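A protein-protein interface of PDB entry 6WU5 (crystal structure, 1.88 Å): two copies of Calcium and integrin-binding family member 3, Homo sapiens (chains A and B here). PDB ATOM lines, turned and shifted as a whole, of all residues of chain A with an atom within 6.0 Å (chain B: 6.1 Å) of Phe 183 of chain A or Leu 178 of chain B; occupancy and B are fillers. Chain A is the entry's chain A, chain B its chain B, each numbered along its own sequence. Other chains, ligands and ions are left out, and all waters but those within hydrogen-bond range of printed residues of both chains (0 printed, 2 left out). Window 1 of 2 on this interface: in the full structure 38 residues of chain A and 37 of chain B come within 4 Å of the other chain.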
ATOM      1  N   ILE A 177      20.170 -17.890  26.238  1.00  0.00           N
ATOM      2  CA  ILE A 177      19.743 -16.873  25.321  1.00  0.00           C
ATOM      3  C   ILE A 177      19.422 -15.619  26.149  1.00  0.00           C
ATOM      4  O   ILE A 177      18.249 -15.289  26.377  1.00  0.00           O
ATOM      5  CB  ILE A 177      18.557 -17.310  24.431  1.00  0.00           C
ATOM      6  CG1 ILE A 177      17.342 -17.747  25.231  1.00  0.00           C
ATOM      7  CG2 ILE A 177      19.010 -18.461  23.539  1.00  0.00           C
ATOM      8  CD1 ILE A 177      16.062 -17.959  24.336  1.00  0.00           C
ATOM      9  N   ALA A 180      17.017 -12.523  24.604  1.00  0.00           N
ATOM     10  CA  ALA A 180      15.801 -12.721  23.816  1.00  0.00           C
ATOM     11  C   ALA A 180      14.615 -12.064  24.514  1.00  0.00           C
ATOM     12  O   ALA A 180      14.529 -12.081  25.749  1.00  0.00           O
ATOM     13  CB  ALA A 180      15.530 -14.208  23.599  1.00  0.00           C
ATOM     14  N   PRO A 181      13.675 -11.501  23.757  1.00  0.00           N
ATOM     15  CA  PRO A 181      12.543 -10.806  24.367  1.00  0.00           C
ATOM     16  C   PRO A 181      11.509 -11.783  24.911  1.00  0.00           C
ATOM     17  O   PRO A 181      11.605 -12.999  24.750  1.00  0.00           O
ATOM     18  CB  PRO A 181      11.977  -9.979  23.210  1.00  0.00           C
ATOM     19  CG  PRO A 181      12.271 -10.816  22.000  1.00  0.00           C
ATOM     20  CD  PRO A 181      13.643 -11.421  22.280  1.00  0.00           C
ATOM     21  N   ASP A 182      10.511 -11.220  25.583  1.00  0.00           N
ATOM     22  CA  ASP A 182       9.390 -11.991  26.113  1.00  0.00           C
ATOM     23  C   ASP A 182       8.461 -12.283  24.940  1.00  0.00           C
ATOM     24  O   ASP A 182       7.654 -11.438  24.548  1.00  0.00           O
ATOM     25  CB  ASP A 182       8.692 -11.207  27.215  1.00  0.00           C
ATOM     26  CG  ASP A 182       7.495 -11.940  27.798  1.00  0.00           C
ATOM     27  OD1 ASP A 182       7.182 -13.063  27.343  1.00  0.00           O
ATOM     28  OD2 ASP A 182       6.868 -11.382  28.721  1.00  0.00           O
ATOM     29  N   PHE A 183       8.591 -13.478  24.358  1.00  0.00           N
ATOM     30  CA  PHE A 183       7.776 -13.828  23.200  1.00  0.00           C
ATOM     31  C   PHE A 183       6.306 -14.038  23.529  1.00  0.00           C
ATOM     32  O   PHE A 183       5.498 -14.153  22.600  1.00  0.00           O
ATOM     33  CB  PHE A 183       8.279 -15.111  22.536  1.00  0.00           C
ATOM     34  CG  PHE A 183       9.612 -14.972  21.898  1.00  0.00           C
ATOM     35  CD1 PHE A 183       9.728 -14.509  20.600  1.00  0.00           C
ATOM     36  CD2 PHE A 183      10.750 -15.292  22.593  1.00  0.00           C
ATOM     37  CE1 PHE A 183      10.966 -14.368  20.013  1.00  0.00           C
ATOM     38  CE2 PHE A 183      11.985 -15.161  22.011  1.00  0.00           C
ATOM     39  CZ  PHE A 183      12.095 -14.693  20.725  1.00  0.00           C
ATOM     40  N   LEU A 184       5.937 -14.136  24.806  1.00  0.00           N
ATOM     41  CA  LEU A 184       4.543 -14.361  25.159  1.00  0.00           C
ATOM     42  C   LEU A 184       3.874 -13.133  25.756  1.00  0.00           C
ATOM     43  O   LEU A 184       2.701 -13.209  26.133  1.00  0.00           O
ATOM     44  CB  LEU A 184       4.428 -15.550  26.123  1.00  0.00           C
ATOM     45  CG  LEU A 184       4.848 -16.903  25.529  1.00  0.00           C
ATOM     46  CD1 LEU A 184       4.710 -18.001  26.579  1.00  0.00           C
ATOM     47  CD2 LEU A 184       4.054 -17.254  24.286  1.00  0.00           C
ATOM     48  N   SER A 185       4.569 -11.993  25.807  1.00  0.00           N
ATOM     49  CA  SER A 185       3.953 -10.769  26.302  1.00  0.00           C
ATOM     50  C   SER A 185       2.686 -10.434  25.535  1.00  0.00           C
ATOM     51  O   SER A 185       1.758  -9.841  26.093  1.00  0.00           O
ATOM     52  CB  SER A 185       4.930  -9.605  26.185  1.00  0.00           C
ATOM     53  OG  SER A 185       5.516  -9.607  24.889  1.00  0.00           O
ATOM     54  N   THR A 186       2.636 -10.794  24.259  1.00  0.00           N
ATOM     55  CA  THR A 186       1.540 -10.428  23.377  1.00  0.00           C
ATOM     56  C   THR A 186       0.290 -11.267  23.582  1.00  0.00           C
ATOM     57  O   THR A 186      -0.684 -11.075  22.845  1.00  0.00           O
ATOM     58  CB  THR A 186       2.007 -10.557  21.924  1.00  0.00           C
ATOM     59  OG1 THR A 186       2.584 -11.855  21.730  1.00  0.00           O
ATOM     60  CG2 THR A 186       3.058  -9.499  21.605  1.00  0.00           C
ATOM     61  N   PHE A 187       0.274 -12.185  24.550  1.00  0.00           N
ATOM     62  CA  PHE A 187      -0.869 -13.078  24.732  1.00  0.00           C
ATOM     63  C   PHE A 187      -1.514 -12.930  26.104  1.00  0.00           C
ATOM     64  O   PHE A 187      -1.936 -13.912  26.719  1.00  0.00           O
ATOM     65  CB  PHE A 187      -0.450 -14.526  24.475  1.00  0.00           C
ATOM     66  CG  PHE A 187      -0.368 -14.859  23.015  1.00  0.00           C
ATOM     67  CD1 PHE A 187      -1.429 -15.463  22.357  1.00  0.00           C
ATOM     68  CD2 PHE A 187       0.757 -14.512  22.290  1.00  0.00           C
ATOM     69  CE1 PHE A 187      -1.353 -15.736  20.998  1.00  0.00           C
ATOM     70  CE2 PHE A 187       0.842 -14.782  20.943  1.00  0.00           C
ATOM     71  CZ  PHE A 187      -0.211 -15.391  20.295  1.00  0.00           C
ATOM     72  N   ARG B 108       0.633 -21.679  30.002  1.00  0.00           N
ATOM     73  CA  ARG B 108       1.765 -21.181  29.228  1.00  0.00           C
ATOM     74  C   ARG B 108       1.900 -21.901  27.892  1.00  0.00           C
ATOM     75  O   ARG B 108       2.107 -21.268  26.850  1.00  0.00           O
ATOM     76  CB  ARG B 108       3.049 -21.336  30.051  1.00  0.00           C
ATOM     77  CG  ARG B 108       4.296 -20.873  29.325  1.00  0.00           C
ATOM     78  CD  ARG B 108       4.957 -22.010  28.566  1.00  0.00           C
ATOM     79  NE  ARG B 108       6.333 -21.708  28.173  1.00  0.00           N
ATOM     80  CZ  ARG B 108       7.051 -22.435  27.320  1.00  0.00           C
ATOM     81  NH1 ARG B 108       6.515 -23.513  26.770  1.00  0.00           N
ATOM     82  NH2 ARG B 108       8.298 -22.096  27.020  1.00  0.00           N
ATOM     83  N   ALA B 112       1.938 -20.417  24.050  1.00  0.00           N
ATOM     84  CA  ALA B 112       3.084 -20.652  23.180  1.00  0.00           C
ATOM     85  C   ALA B 112       2.662 -21.323  21.878  1.00  0.00           C
ATOM     86  O   ALA B 112       3.210 -21.031  20.809  1.00  0.00           O
ATOM     87  CB  ALA B 112       4.123 -21.501  23.907  1.00  0.00           C
ATOM     88  N   ALA B 115       1.327 -18.460  19.953  1.00  0.00           N
ATOM     89  CA  ALA B 115       2.428 -17.567  19.601  1.00  0.00           C
ATOM     90  C   ALA B 115       3.203 -18.112  18.405  1.00  0.00           C
ATOM     91  O   ALA B 115       3.534 -17.368  17.474  1.00  0.00           O
ATOM     92  CB  ALA B 115       3.360 -17.377  20.799  1.00  0.00           C
ATOM     93  N   TYR B 119       3.776 -15.827  14.947  1.00  0.00           N
ATOM     94  CA  TYR B 119       5.126 -15.503  14.506  1.00  0.00           C
ATOM     95  C   TYR B 119       5.550 -16.292  13.272  1.00  0.00           C
ATOM     96  O   TYR B 119       6.579 -15.964  12.669  1.00  0.00           O
ATOM     97  CB  TYR B 119       6.137 -15.752  15.631  1.00  0.00           C
ATOM     98  CG  TYR B 119       5.848 -14.983  16.900  1.00  0.00           C
ATOM     99  CD1 TYR B 119       5.321 -13.701  16.849  1.00  0.00           C
ATOM    100  CD2 TYR B 119       6.098 -15.545  18.147  1.00  0.00           C
ATOM    101  CE1 TYR B 119       5.032 -12.997  18.011  1.00  0.00           C
ATOM    102  CE2 TYR B 119       5.829 -14.841  19.315  1.00  0.00           C
ATOM    103  CZ  TYR B 119       5.300 -13.569  19.235  1.00  0.00           C
ATOM    104  OH  TYR B 119       5.033 -12.864  20.390  1.00  0.00           O
ATOM    105  N   LEU B 132      11.792 -15.045  12.532  1.00  0.00           N
ATOM    106  CA  LEU B 132      12.377 -14.700  13.822  1.00  0.00           C
ATOM    107  C   LEU B 132      12.845 -13.251  13.842  1.00  0.00           C
ATOM    108  O   LEU B 132      12.619 -12.530  14.822  1.00  0.00           O
ATOM    109  CB  LEU B 132      13.535 -15.642  14.134  1.00  0.00           C
ATOM    110  CG  LEU B 132      14.121 -15.577  15.541  1.00  0.00           C
ATOM    111  CD1 LEU B 132      13.058 -15.854  16.580  1.00  0.00           C
ATOM    112  CD2 LEU B 132      15.270 -16.562  15.687  1.00  0.00           C
ATOM    113  N   THR B 135       9.896 -10.929  14.149  1.00  0.00           N
ATOM    114  CA  THR B 135       9.276 -11.026  15.464  1.00  0.00           C
ATOM    115  C   THR B 135      10.097 -10.288  16.510  1.00  0.00           C
ATOM    116  O   THR B 135       9.567  -9.469  17.269  1.00  0.00           O
ATOM    117  CB  THR B 135       9.137 -12.498  15.873  1.00  0.00           C
ATOM    118  OG1 THR B 135       8.210 -13.160  15.004  1.00  0.00           O
ATOM    119  CG2 THR B 135       8.657 -12.612  17.313  1.00  0.00           C
ATOM    120  N   VAL B 136      11.386 -10.594  16.592  1.00  0.00           N
ATOM    121  CA  VAL B 136      12.215  -9.969  17.617  1.00  0.00           C
ATOM    122  C   VAL B 136      12.291  -8.471  17.380  1.00  0.00           C
ATOM    123  O   VAL B 136      12.231  -7.675  18.324  1.00  0.00           O
ATOM    124  CB  VAL B 136      13.600 -10.631  17.645  1.00  0.00           C
ATOM    125  CG1 VAL B 136      14.572  -9.866  18.544  1.00  0.00           C
ATOM    126  CG2 VAL B 136      13.469 -12.069  18.127  1.00  0.00           C
ATOM    127  N   LEU B 139       9.130  -6.896  18.733  1.00  0.00           N
ATOM    128  CA  LEU B 139       9.066  -6.969  20.185  1.00  0.00           C
ATOM    129  C   LEU B 139      10.079  -6.059  20.880  1.00  0.00           C
ATOM    130  O   LEU B 139       9.947  -5.823  22.087  1.00  0.00           O
ATOM    131  CB  LEU B 139       9.284  -8.420  20.640  1.00  0.00           C
ATOM    132  CG  LEU B 139       8.167  -9.416  20.294  1.00  0.00           C
ATOM    133  CD1 LEU B 139       8.606 -10.855  20.478  1.00  0.00           C
ATOM    134  CD2 LEU B 139       6.949  -9.131  21.147  1.00  0.00           C
ATOM    135  N   VAL B 152      20.774 -11.675  18.433  1.00  0.00           N
ATOM    136  CA  VAL B 152      19.802 -12.461  19.191  1.00  0.00           C
ATOM    137  C   VAL B 152      19.250 -13.587  18.325  1.00  0.00           C
ATOM    138  O   VAL B 152      19.167 -14.746  18.749  1.00  0.00           O
ATOM    139  CB  VAL B 152      18.669 -11.565  19.720  1.00  0.00           C
ATOM    140  CG1 VAL B 152      17.512 -12.427  20.216  1.00  0.00           C
ATOM    141  CG2 VAL B 152      19.183 -10.665  20.818  1.00  0.00           C
ATOM    142  N   VAL B 156      19.544 -17.630  19.128  1.00  0.00           N
ATOM    143  CA  VAL B 156      18.323 -18.407  19.308  1.00  0.00           C
ATOM    144  C   VAL B 156      18.344 -19.611  18.376  1.00  0.00           C
ATOM    145  O   VAL B 156      18.132 -20.754  18.796  1.00  0.00           O
ATOM    146  CB  VAL B 156      17.087 -17.525  19.072  1.00  0.00           C
ATOM    147  CG1 VAL B 156      15.857 -18.404  18.894  1.00  0.00           C
ATOM    148  CG2 VAL B 156      16.899 -16.537  20.223  1.00  0.00           C
ATOM    149  N   PHE B 173      10.279 -24.249  19.783  1.00  0.00           N
ATOM    150  CA  PHE B 173       9.757 -23.016  20.362  1.00  0.00           C
ATOM    151  C   PHE B 173       9.234 -23.251  21.774  1.00  0.00           C
ATOM    152  O   PHE B 173       9.521 -22.472  22.691  1.00  0.00           O
ATOM    153  CB  PHE B 173       8.670 -22.468  19.437  1.00  0.00           C
ATOM    154  CG  PHE B 173       8.197 -21.097  19.779  1.00  0.00           C
ATOM    155  CD1 PHE B 173       8.969 -19.991  19.491  1.00  0.00           C
ATOM    156  CD2 PHE B 173       6.959 -20.908  20.364  1.00  0.00           C
ATOM    157  CE1 PHE B 173       8.517 -18.724  19.791  1.00  0.00           C
ATOM    158  CE2 PHE B 173       6.514 -19.633  20.682  1.00  0.00           C
ATOM    159  CZ  PHE B 173       7.289 -18.547  20.384  1.00  0.00           C
ATOM    160  N   GLN B 174       8.465 -24.329  21.964  1.00  0.00           N
ATOM    161  CA  GLN B 174       7.918 -24.642  23.278  1.00  0.00           C
ATOM    162  C   GLN B 174       9.006 -24.810  24.332  1.00  0.00           C
ATOM    163  O   GLN B 174       8.810 -24.449  25.499  1.00  0.00           O
ATOM    164  CB  GLN B 174       7.084 -25.915  23.190  1.00  0.00           C
ATOM    165  CG  GLN B 174       5.803 -25.744  22.421  1.00  0.00           C
ATOM    166  CD  GLN B 174       4.703 -25.232  23.303  1.00  0.00           C
ATOM    167  OE1 GLN B 174       4.963 -24.761  24.413  1.00  0.00           O
ATOM    168  NE2 GLN B 174       3.460 -25.332  22.834  1.00  0.00           N
ATOM    169  N   ASN B 175      10.149 -25.373  23.950  1.00  0.00           N
ATOM    170  CA  ASN B 175      11.215 -25.643  24.907  1.00  0.00           C
ATOM    171  C   ASN B 175      12.059 -24.420  25.241  1.00  0.00           C
ATOM    172  O   ASN B 175      12.897 -24.500  26.147  1.00  0.00           O
ATOM    173  CB  ASN B 175      12.129 -26.742  24.360  1.00  0.00           C
ATOM    174  CG  ASN B 175      11.559 -28.117  24.565  1.00  0.00           C
ATOM    175  OD1 ASN B 175      11.223 -28.501  25.684  1.00  0.00           O
ATOM    176  ND2 ASN B 175      11.441 -28.876  23.481  1.00  0.00           N
ATOM    177  N   MET B 176      11.862 -23.301  24.548  1.00  0.00           N
ATOM    178  CA  MET B 176      12.668 -22.115  24.785  1.00  0.00           C
ATOM    179  C   MET B 176      12.253 -21.416  26.080  1.00  0.00           C
ATOM    180  O   MET B 176      11.120 -21.553  26.561  1.00  0.00           O
ATOM    181  CB  MET B 176      12.524 -21.133  23.622  1.00  0.00           C
ATOM    182  CG  MET B 176      13.501 -21.372  22.489  1.00  0.00           C
ATOM    183  SD  MET B 176      12.972 -20.605  20.953  1.00  0.00           S
ATOM    184  CE  MET B 176      13.260 -18.880  21.277  1.00  0.00           C
ATOM    185  N   ILE B 177      13.190 -20.642  26.641  1.00  0.00           N
ATOM    186  CA  ILE B 177      12.896 -19.762  27.776  1.00  0.00           C
ATOM    187  C   ILE B 177      12.225 -18.507  27.230  1.00  0.00           C
ATOM    188  O   ILE B 177      12.797 -17.413  27.233  1.00  0.00           O
ATOM    189  CB  ILE B 177      14.173 -19.474  28.596  1.00  0.00           C
ATOM    190  CG1 ILE B 177      15.255 -18.775  27.774  1.00  0.00           C
ATOM    191  CG2 ILE B 177      14.694 -20.793  29.175  1.00  0.00           C
ATOM    192  CD1 ILE B 177      16.581 -18.496  28.547  1.00  0.00           C
ATOM    193  N   LEU B 178      10.962 -18.661  26.812  1.00  0.00           N
ATOM    194  CA  LEU B 178      10.265 -17.666  26.006  1.00  0.00           C
ATOM    195  C   LEU B 178      10.039 -16.319  26.690  1.00  0.00           C
ATOM    196  O   LEU B 178       9.852 -15.317  25.987  1.00  0.00           O
ATOM    197  CB  LEU B 178       8.910 -18.252  25.588  1.00  0.00           C
ATOM    198  CG  LEU B 178       8.996 -19.443  24.635  1.00  0.00           C
ATOM    199  CD1 LEU B 178       7.621 -20.111  24.468  1.00  0.00           C
ATOM    200  CD2 LEU B 178       9.546 -18.989  23.294  1.00  0.00           C
ATOM    201  N   ARG B 179      10.000 -16.266  28.028  1.00  0.00           N
ATOM    202  CA  ARG B 179       9.631 -15.023  28.699  1.00  0.00           C
ATOM    203  C   ARG B 179      10.759 -14.462  29.558  1.00  0.00           C
ATOM    204  O   ARG B 179      10.514 -13.545  30.355  1.00  0.00           O
ATOM    205  CB  ARG B 179       8.402 -15.234  29.589  1.00  0.00           C
ATOM    206  CG  ARG B 179       7.191 -15.886  28.894  1.00  0.00           C
ATOM    207  CD  ARG B 179       5.912 -15.548  29.627  1.00  0.00           C
ATOM    208  NE  ARG B 179       5.624 -14.128  29.501  1.00  0.00           N
ATOM    209  CZ  ARG B 179       4.652 -13.500  30.140  1.00  0.00           C
ATOM    210  NH1 ARG B 179       3.848 -14.169  30.968  1.00  0.00           N
ATOM    211  NH2 ARG B 179       4.491 -12.200  29.951  1.00  0.00           N
ATOM    212  N   ALA B 180      11.954 -15.012  29.455  1.00  0.00           N
ATOM    213  CA  ALA B 180      13.062 -14.537  30.273  1.00  0.00           C
ATOM    214  C   ALA B 180      13.456 -13.130  29.837  1.00  0.00           C
ATOM    215  O   ALA B 180      13.451 -12.825  28.641  1.00  0.00           O
ATOM    216  CB  ALA B 180      14.259 -15.476  30.159  1.00  0.00           C
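The side-chain carboxylate of Asp 182 of chain A is in salt-bridge range of the guanidinium group of Arg 179 of chain B (2.8 Å). The side-chain hydroxyl (OH) of Tyr 119 of chain B sits at hydrogen-bond distance from the backbone carbonyl oxygen (O) of Phe 183 of chain A. N of Phe 183 of chain A lies within hydrogen-bond range of O of Leu 178 of chain B. OG1 of Thr 186 of chain A is in hydrogen-bond range of OH of Tyr 119 of chain B (3.0 Å). The backbone carbonyl oxygen (O) of Ala 180 of chain A sits close to the backbone carbonyl oxygen (O) of Ala 180 of chain B (3.2 Å). O of Pro 181 of chain A lies close to O of Leu 178 of chain B.
The side-chain carboxylate (OD1) of Asp 182 of chain A is in hydrogen-bond range of the backbone NH (N) of Leu 184 of chain A (3.0 Å). OG of Ser 185 of chain A sits at hydrogen-bond distance from O of Asp 182 of chain A (2.8 Å). The backbone carbonyl oxygen (O) of Gln 174 of chain B sits at hydrogen-bond distance from the guanidinium group (NH1) of Arg 108 of chain B, at 2.8 Å. The backbone carbonyl oxygen of Met 176 of chain B sits at hydrogen-bond distance from the guanidinium group of Arg 108 of chain B, 2.9 Å away.
Among the printed residues, merely in contact across the chains: Asp 182 of chain A with Leu 178 of chain B, Ile 177 of chain A with Ile 177 of chain B, Phe 187 of chain A with Ala 115 of chain B, Leu 184 of chain A with Ala 115 of chain B, Leu 184 of chain A with Ala 112 of chain B, Leu 184 of chain A with Arg 179 of chain B, Phe 183 of chain A with Leu 139 of chain B, Phe 183 of chain A with Val 136 of chain B, Thr 186 of chain A with Leu 139 of chain B, Phe 183 of chain A with Thr 135 of chain B, Ser 185 of chain A with Arg 179 of chain B, Pro 181 of chain A with Leu 139 of chain B, Leu 184 of chain A with Arg 108 of chain B, Ala 180 of chain A with Val 152 of chain B and Phe 183 of chain A with Met 176 of chain B.
Of the printed residues of chain B, Phe 183 of chain A touches Tyr 119 (2.6 Å), Thr 135 (3.9 Å), Val 136 (3.9 Å), Leu 139 (3.8 Å), Met 176 (3.999 Å) and Leu 178 (2.8 Å). Leu 178 of chain B touches three residues of chain A. Of the printed residues of chain B, Asp 182 of chain A touches Leu 178 and Arg 179. Printed residues of chain A within 4 Å of Ala 115 of chain B: Leu 184 and Phe 187. Printed residues of chain A within 4 Å of Val 136 of chain B: Phe 183. Printed residues of chain B within 4 Å of Ile 177 of chain A: Ile 177 (3.4 Å). Of the printed residues of chain A, Leu 139 of chain B touches Pro 181 (3.97 Å), Phe 183 (3.8 Å) and Thr 186 (3.9 Å). The nearest printed residue of chain B that does not touch Phe 187 of chain A is Tyr 119 of chain B (4.6 Å).
Of the 18 printed residues of chain B, 13 touch a printed residue of chain A. Printed residues of chain B that touch a printed residue of chain A: Arg 108, Ala 112, Ala 115, Tyr 119, Thr 135, Val 136, Leu 139, Val 152, Met 176, Ile 177, Leu 178, Arg 179 and Ala 180. Hydrophobic or aromatic side chains of chain B that line the printed part of chain A: Ala 115, Tyr 119, Val 136, Leu 139, Val 152, Met 176, Ile 177 and Leu 178. Of the 9 printed residues of chain A, 9 touch a printed residue of chain B. Printed residues of chain A that touch a printed residue of chain B: Ile 177, Ala 180, Pro 181, Asp 182, Phe 183, Leu 184, Ser 185, Thr 186 and Phe 187. Hydrophobic or aromatic side chains of chain A within 4 Å of the printed part of chain B: Ile 177, Pro 181, Phe 183, Leu 184 and Phe 187. Among the printed residues, 21 pairs touch across the chains.
Ile 177 of chain B touches its own counterpart, Ile 177 of chain A. Ala 180 of chain A touches its own counterpart, Ala 180 of chain B. 2 positions are printed for both chains.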
